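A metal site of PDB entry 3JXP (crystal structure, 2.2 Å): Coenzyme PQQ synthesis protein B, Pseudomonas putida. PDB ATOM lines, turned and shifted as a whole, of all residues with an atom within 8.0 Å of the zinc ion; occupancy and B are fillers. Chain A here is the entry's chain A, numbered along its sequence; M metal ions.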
ATOM      1  N   GLY A  15     -27.072  -5.683  -5.412  1.00  0.00           N
ATOM      2  CA  GLY A  15     -28.531  -5.847  -5.204  1.00  0.00           C
ATOM      3  C   GLY A  15     -28.919  -7.292  -5.485  1.00  0.00           C
ATOM      4  O   GLY A  15     -28.070  -8.158  -5.692  1.00  0.00           O
ATOM      5  N   PHE A  16     -30.213  -7.574  -5.496  1.00  0.00           N
ATOM      6  CA  PHE A  16     -30.689  -8.914  -5.839  1.00  0.00           C
ATOM      7  C   PHE A  16     -31.993  -8.842  -6.627  1.00  0.00           C
ATOM      8  O   PHE A  16     -32.930  -8.222  -6.149  1.00  0.00           O
ATOM      9  CB  PHE A  16     -30.912  -9.775  -4.583  1.00  0.00           C
ATOM     10  CG  PHE A  16     -31.607 -11.054  -4.881  1.00  0.00           C
ATOM     11  CD1 PHE A  16     -30.949 -12.039  -5.644  1.00  0.00           C
ATOM     12  CD2 PHE A  16     -32.928 -11.253  -4.506  1.00  0.00           C
ATOM     13  CE1 PHE A  16     -31.604 -13.227  -5.958  1.00  0.00           C
ATOM     14  CE2 PHE A  16     -33.573 -12.430  -4.830  1.00  0.00           C
ATOM     15  CZ  PHE A  16     -32.895 -13.410  -5.561  1.00  0.00           C
ATOM     16  N   PRO A  17     -32.041  -9.368  -7.892  1.00  0.00           N
ATOM     17  CA  PRO A  17     -30.940  -9.983  -8.694  1.00  0.00           C
ATOM     18  C   PRO A  17     -29.938  -8.909  -9.080  1.00  0.00           C
ATOM     19  O   PRO A  17     -30.294  -7.683  -9.144  1.00  0.00           O
ATOM     20  CB  PRO A  17     -31.656 -10.508  -9.971  1.00  0.00           C
ATOM     21  CG  PRO A  17     -32.937  -9.665 -10.091  1.00  0.00           C
ATOM     22  CD  PRO A  17     -33.294  -9.197  -8.662  1.00  0.00           C
ATOM     23  N   GLN A  18     -28.689  -9.325  -9.288  1.00  0.00           N
ATOM     24  CA  GLN A  18     -27.669  -8.432  -9.748  1.00  0.00           C
ATOM     25  C   GLN A  18     -27.730  -8.345 -11.284  1.00  0.00           C
ATOM     26  O   GLN A  18     -27.954  -9.367 -11.989  1.00  0.00           O
ATOM     27  CB  GLN A  18     -26.300  -8.842  -9.181  1.00  0.00           C
ATOM     28  CG  GLN A  18     -25.104  -8.107  -9.748  1.00  0.00           C
ATOM     29  CD  GLN A  18     -23.824  -8.444  -9.037  1.00  0.00           C
ATOM     30  OE1 GLN A  18     -23.777  -8.554  -7.824  1.00  0.00           O
ATOM     31  NE2 GLN A  18     -22.743  -8.592  -9.795  1.00  0.00           N
ATOM     32  N   TRP A  19     -27.576  -7.126 -11.799  1.00  0.00           N
ATOM     33  CA  TRP A  19     -27.778  -6.799 -13.213  1.00  0.00           C
ATOM     34  C   TRP A  19     -27.081  -7.760 -14.192  1.00  0.00           C
ATOM     35  O   TRP A  19     -27.655  -8.095 -15.215  1.00  0.00           O
ATOM     36  CB  TRP A  19     -27.328  -5.330 -13.513  1.00  0.00           C
ATOM     37  CG  TRP A  19     -25.824  -5.155 -13.497  1.00  0.00           C
ATOM     38  CD1 TRP A  19     -25.021  -5.068 -12.397  1.00  0.00           C
ATOM     39  CD2 TRP A  19     -24.952  -5.097 -14.636  1.00  0.00           C
ATOM     40  NE1 TRP A  19     -23.716  -4.943 -12.765  1.00  0.00           N
ATOM     41  CE2 TRP A  19     -23.635  -4.961 -14.129  1.00  0.00           C
ATOM     42  CE3 TRP A  19     -25.151  -5.131 -16.028  1.00  0.00           C
ATOM     43  CZ2 TRP A  19     -22.520  -4.887 -14.960  1.00  0.00           C
ATOM     44  CZ3 TRP A  19     -24.036  -5.057 -16.859  1.00  0.00           C
ATOM     45  CH2 TRP A  19     -22.752  -4.906 -16.329  1.00  0.00           C
ATOM     46  N   ASN A  20     -25.856  -8.177 -13.894  1.00  0.00           N
ATOM     47  CA  ASN A  20     -25.080  -9.005 -14.825  1.00  0.00           C
ATOM     48  C   ASN A  20     -24.906 -10.458 -14.346  1.00  0.00           C
ATOM     49  O   ASN A  20     -24.075 -11.222 -14.881  1.00  0.00           O
ATOM     50  CB  ASN A  20     -23.702  -8.363 -15.126  1.00  0.00           C
ATOM     51  CG  ASN A  20     -22.792  -8.389 -13.927  1.00  0.00           C
ATOM     52  OD1 ASN A  20     -23.240  -8.502 -12.794  1.00  0.00           O
ATOM     53  ND2 ASN A  20     -21.478  -8.284 -14.174  1.00  0.00           N
ATOM     54  N   CYS A  21     -25.697 -10.840 -13.349  1.00  0.00           N
ATOM     55  CA  CYS A  21     -25.510 -12.115 -12.683  1.00  0.00           C
ATOM     56  C   CYS A  21     -26.521 -13.162 -13.091  1.00  0.00           C
ATOM     57  O   CYS A  21     -27.729 -12.950 -13.047  1.00  0.00           O
ATOM     58  CB  CYS A  21     -25.423 -11.967 -11.148  1.00  0.00           C
ATOM     59  SG  CYS A  21     -24.932 -13.526 -10.335  1.00  0.00           S
ATOM     60  N   ASN A  22     -26.026 -14.333 -13.480  1.00  0.00           N
ATOM     61  CA  ASN A  22     -26.965 -15.476 -13.667  1.00  0.00           C
ATOM     62  C   ASN A  22     -26.678 -16.661 -12.734  1.00  0.00           C
ATOM     63  O   ASN A  22     -26.835 -17.817 -13.133  1.00  0.00           O
ATOM     64  CB  ASN A  22     -26.984 -15.947 -15.134  1.00  0.00           C
ATOM     65  CG  ASN A  22     -27.288 -14.833 -16.102  1.00  0.00           C
ATOM     66  OD1 ASN A  22     -28.449 -14.463 -16.322  1.00  0.00           O
ATOM     67  ND2 ASN A  22     -26.236 -14.291 -16.706  1.00  0.00           N
ATOM     68  N   CYS A  23     -26.213 -16.386 -11.517  1.00  0.00           N
ATOM     69  CA  CYS A  23     -25.980 -17.413 -10.501  1.00  0.00           C
ATOM     70  C   CYS A  23     -27.287 -18.127 -10.188  1.00  0.00           C
ATOM     71  O   CYS A  23     -28.343 -17.748 -10.719  1.00  0.00           O
ATOM     72  CB  CYS A  23     -25.336 -16.844  -9.216  1.00  0.00           C
ATOM     73  SG  CYS A  23     -26.556 -16.112  -7.963  1.00  0.00           S
ATOM     74  N   VAL A  24     -27.233 -19.162  -9.337  1.00  0.00           N
ATOM     75  CA  VAL A  24     -28.447 -19.945  -9.047  1.00  0.00           C
ATOM     76  C   VAL A  24     -29.563 -19.071  -8.479  1.00  0.00           C
ATOM     77  O   VAL A  24     -30.737 -19.253  -8.824  1.00  0.00           O
ATOM     78  CB  VAL A  24     -28.184 -21.232  -8.182  1.00  0.00           C
ATOM     79  CG1 VAL A  24     -27.115 -22.075  -8.794  1.00  0.00           C
ATOM     80  CG2 VAL A  24     -27.787 -20.895  -6.775  1.00  0.00           C
ATOM     81  N   ASN A  25     -29.225 -18.101  -7.632  1.00  0.00           N
ATOM     82  CA  ASN A  25     -30.247 -17.224  -7.038  1.00  0.00           C
ATOM     83  C   ASN A  25     -30.853 -16.265  -8.062  1.00  0.00           C
ATOM     84  O   ASN A  25     -32.057 -16.160  -8.170  1.00  0.00           O
ATOM     85  CB  ASN A  25     -29.719 -16.455  -5.804  1.00  0.00           C
ATOM     86  CG  ASN A  25     -29.576 -17.337  -4.561  1.00  0.00           C
ATOM     87  OD1 ASN A  25     -30.182 -18.405  -4.479  1.00  0.00           O
ATOM     88  ND2 ASN A  25     -28.783 -16.888  -3.580  1.00  0.00           N
ATOM     89  N   CYS A  26     -30.007 -15.560  -8.813  1.00  0.00           N
ATOM     90  CA  CYS A  26     -30.520 -14.508  -9.711  1.00  0.00           C
ATOM     91  C   CYS A  26     -31.214 -15.106 -10.922  1.00  0.00           C
ATOM     92  O   CYS A  26     -32.284 -14.614 -11.341  1.00  0.00           O
ATOM     93  CB  CYS A  26     -29.403 -13.570 -10.172  1.00  0.00           C
ATOM     94  SG  CYS A  26     -28.435 -12.814  -8.887  1.00  0.00           S
ATOM     95  N   LYS A  27     -30.590 -16.123 -11.515  1.00  0.00           N
ATOM     96  CA  LYS A  27     -31.262 -16.855 -12.608  1.00  0.00           C
ATOM     97  C   LYS A  27     -32.584 -17.426 -12.139  1.00  0.00           C
ATOM     98  O   LYS A  27     -33.618 -17.263 -12.813  1.00  0.00           O
ATOM     99  CB  LYS A  27     -30.390 -17.974 -13.181  1.00  0.00           C
ATOM    100  CG  LYS A  27     -30.947 -18.539 -14.504  1.00  0.00           C
ATOM    101  CD  LYS A  27     -29.895 -19.379 -15.210  1.00  0.00           C
ATOM    102  CE  LYS A  27     -29.946 -19.177 -16.736  1.00  0.00           C
ATOM    103  NZ  LYS A  27     -31.022 -19.945 -17.459  1.00  0.00           N
ATOM    104  N   GLY A  28     -32.568 -18.073 -10.976  1.00  0.00           N
ATOM    105  CA  GLY A  28     -33.786 -18.735 -10.474  1.00  0.00           C
ATOM    106  C   GLY A  28     -34.844 -17.694 -10.180  1.00  0.00           C
ATOM    107  O   GLY A  28     -36.013 -17.932 -10.460  1.00  0.00           O
ATOM    108  N   ARG A  30     -35.191 -14.887 -11.789  1.00  0.00           N
ATOM    109  CA  ARG A  30     -35.726 -14.379 -13.068  1.00  0.00           C
ATOM    110  C   ARG A  30     -36.579 -15.426 -13.780  1.00  0.00           C
ATOM    111  O   ARG A  30     -37.561 -15.076 -14.435  1.00  0.00           O
ATOM    112  CB  ARG A  30     -34.606 -13.894 -14.012  1.00  0.00           C
ATOM    113  CG  ARG A  30     -33.900 -12.564 -13.609  1.00  0.00           C
ATOM    114  CD  ARG A  30     -32.866 -12.170 -14.659  1.00  0.00           C
ATOM    115  NE  ARG A  30     -31.848 -11.305 -14.072  1.00  0.00           N
ATOM    116  CZ  ARG A  30     -30.614 -11.695 -13.765  1.00  0.00           C
ATOM    117  NH1 ARG A  30     -29.801 -10.822 -13.190  1.00  0.00           N
ATOM    118  NH2 ARG A  30     -30.195 -12.937 -14.025  1.00  0.00           N
ATOM    119  N   ARG A 234     -20.393 -20.459  -6.359  1.00  0.00           N
ATOM    120  CA  ARG A 234     -21.451 -20.065  -7.276  1.00  0.00           C
ATOM    121  C   ARG A 234     -20.947 -19.881  -8.720  1.00  0.00           C
ATOM    122  O   ARG A 234     -21.743 -19.926  -9.652  1.00  0.00           O
ATOM    123  CB  ARG A 234     -22.180 -18.789  -6.790  1.00  0.00           C
ATOM    124  CG  ARG A 234     -22.750 -18.836  -5.357  1.00  0.00           C
ATOM    125  CD  ARG A 234     -23.617 -20.036  -5.067  1.00  0.00           C
ATOM    126  NE  ARG A 234     -24.788 -19.693  -4.270  1.00  0.00           N
ATOM    127  CZ  ARG A 234     -25.734 -20.557  -3.911  1.00  0.00           C
ATOM    128  NH1 ARG A 234     -26.791 -20.155  -3.212  1.00  0.00           N
ATOM    129  NH2 ARG A 234     -25.617 -21.834  -4.257  1.00  0.00           N
ATOM    130  N   VAL A 236     -18.988 -17.109  -9.731  1.00  0.00           N
ATOM    131  CA  VAL A 236     -19.180 -15.699 -10.126  1.00  0.00           C
ATOM    132  C   VAL A 236     -18.038 -14.775  -9.715  1.00  0.00           C
ATOM    133  O   VAL A 236     -18.110 -13.565  -9.894  1.00  0.00           O
ATOM    134  CB  VAL A 236     -20.515 -15.134  -9.603  1.00  0.00           C
ATOM    135  CG1 VAL A 236     -21.696 -15.920 -10.194  1.00  0.00           C
ATOM    136  CG2 VAL A 236     -20.550 -15.131  -8.069  1.00  0.00           C
ATOM    137  N   ASN A 273     -25.672 -10.888   0.141  1.00  0.00           N
ATOM    138  CA  ASN A 273     -25.214 -11.009  -1.238  1.00  0.00           C
ATOM    139  C   ASN A 273     -26.198 -11.810  -2.058  1.00  0.00           C
ATOM    140  O   ASN A 273     -26.908 -12.655  -1.530  1.00  0.00           O
ATOM    141  CB  ASN A 273     -23.774 -11.542  -1.355  1.00  0.00           C
ATOM    142  CG  ASN A 273     -23.064 -11.046  -2.651  1.00  0.00           C
ATOM    143  OD1 ASN A 273     -22.943  -9.835  -2.901  1.00  0.00           O
ATOM    144  ND2 ASN A 273     -22.584 -11.985  -3.471  1.00  0.00           N
ATOM    145  N   ASN A 274     -26.244 -11.506  -3.360  1.00  0.00           N
ATOM    146  CA  ASN A 274     -27.143 -12.148  -4.319  1.00  0.00           C
ATOM    147  C   ASN A 274     -26.930 -13.657  -4.392  1.00  0.00           C
ATOM    148  O   ASN A 274     -27.847 -14.390  -4.708  1.00  0.00           O
ATOM    149  CB  ASN A 274     -27.006 -11.496  -5.694  1.00  0.00           C
ATOM    150  CG  ASN A 274     -25.638 -11.762  -6.358  1.00  0.00           C
ATOM    151  OD1 ASN A 274     -25.434 -12.803  -7.011  1.00  0.00           O
ATOM    152  ND2 ASN A 274     -24.702 -10.836  -6.178  1.00  0.00           N
ATOM    153  N   THR A 275     -25.699 -14.085  -4.100  1.00  0.00           N
ATOM    154  CA  THR A 275     -25.308 -15.508  -4.043  1.00  0.00           C
ATOM    155  C   THR A 275     -25.600 -16.214  -2.713  1.00  0.00           C
ATOM    156  O   THR A 275     -25.422 -17.439  -2.636  1.00  0.00           O
ATOM    157  CB  THR A 275     -23.800 -15.676  -4.237  1.00  0.00           C
ATOM    158  OG1 THR A 275     -23.110 -14.855  -3.266  1.00  0.00           O
ATOM    159  CG2 THR A 275     -23.378 -15.296  -5.687  1.00  0.00           C
ATOM    160  N   ASN A 276     -26.049 -15.476  -1.684  1.00  0.00           N
ATOM    161  CA  ASN A 276     -26.392 -16.101  -0.378  1.00  0.00           C
ATOM    162  C   ASN A 276     -27.668 -16.997  -0.425  1.00  0.00           C
ATOM    163  O   ASN A 276     -28.761 -16.511  -0.733  1.00  0.00           O
ATOM    164  CB  ASN A 276     -26.476 -15.043   0.749  1.00  0.00           C
ATOM    165  CG  ASN A 276     -26.297 -15.626   2.156  1.00  0.00           C
ATOM    166  OD1 ASN A 276     -26.676 -16.748   2.403  1.00  0.00           O
ATOM    167  ND2 ASN A 276     -25.700 -14.856   3.071  1.00  0.00           N
ATOM    168  N   LEU A 279     -31.329 -16.314   0.834  1.00  0.00           N
ATOM    169  CA  LEU A 279     -32.300 -15.575  -0.009  1.00  0.00           C
ATOM    170  C   LEU A 279     -33.387 -16.478  -0.543  1.00  0.00           C
ATOM    171  O   LEU A 279     -34.544 -16.041  -0.770  1.00  0.00           O
ATOM    172  CB  LEU A 279     -31.601 -14.840  -1.178  1.00  0.00           C
ATOM    173  CG  LEU A 279     -30.763 -13.605  -0.826  1.00  0.00           C
ATOM    174  CD1 LEU A 279     -30.178 -12.938  -2.075  1.00  0.00           C
ATOM    175  CD2 LEU A 279     -31.572 -12.595   0.019  1.00  0.00           C
HETATM  176 ZN    ZN M   1     -26.377 -13.775  -8.613  1.00  0.00          ZN
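OD1 of Asn 274 binds the zinc ion (2.1 Å). The side-chain sulfur (SG) of Cys 21 is bound to the zinc ion (2.3 Å). The zinc ion is bound by SG of Cys 26. The side-chain sulfur (SG) of Cys 23 binds the zinc ion, at 2.4 Å. The zinc ion has four donor atoms within binding distance.
The side-chain amide oxygen (OE1) of Gln 18 lies within hydrogen-bond range of the side-chain amide nitrogen (ND2) of Asn 274, at 3.0 Å. ND2 of Asn 25 is in hydrogen-bond range of O of Asn 274, 2.9 Å away. NH2 of Arg 30 sits at hydrogen-bond distance from O of Cys 21, 2.7 Å away. SG of Cys 26 sits close to N of Gln 18 (3.5 Å). N of Asn 25 lies close to SG of Cys 23 (3.3 Å).
Four residues have an atom within 4 Å of the zinc ion: Cys 21, Cys 23, Cys 26 and Asn 274. Along chain A the residues within 4 Å of the zinc ion span positions 21 to 274.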
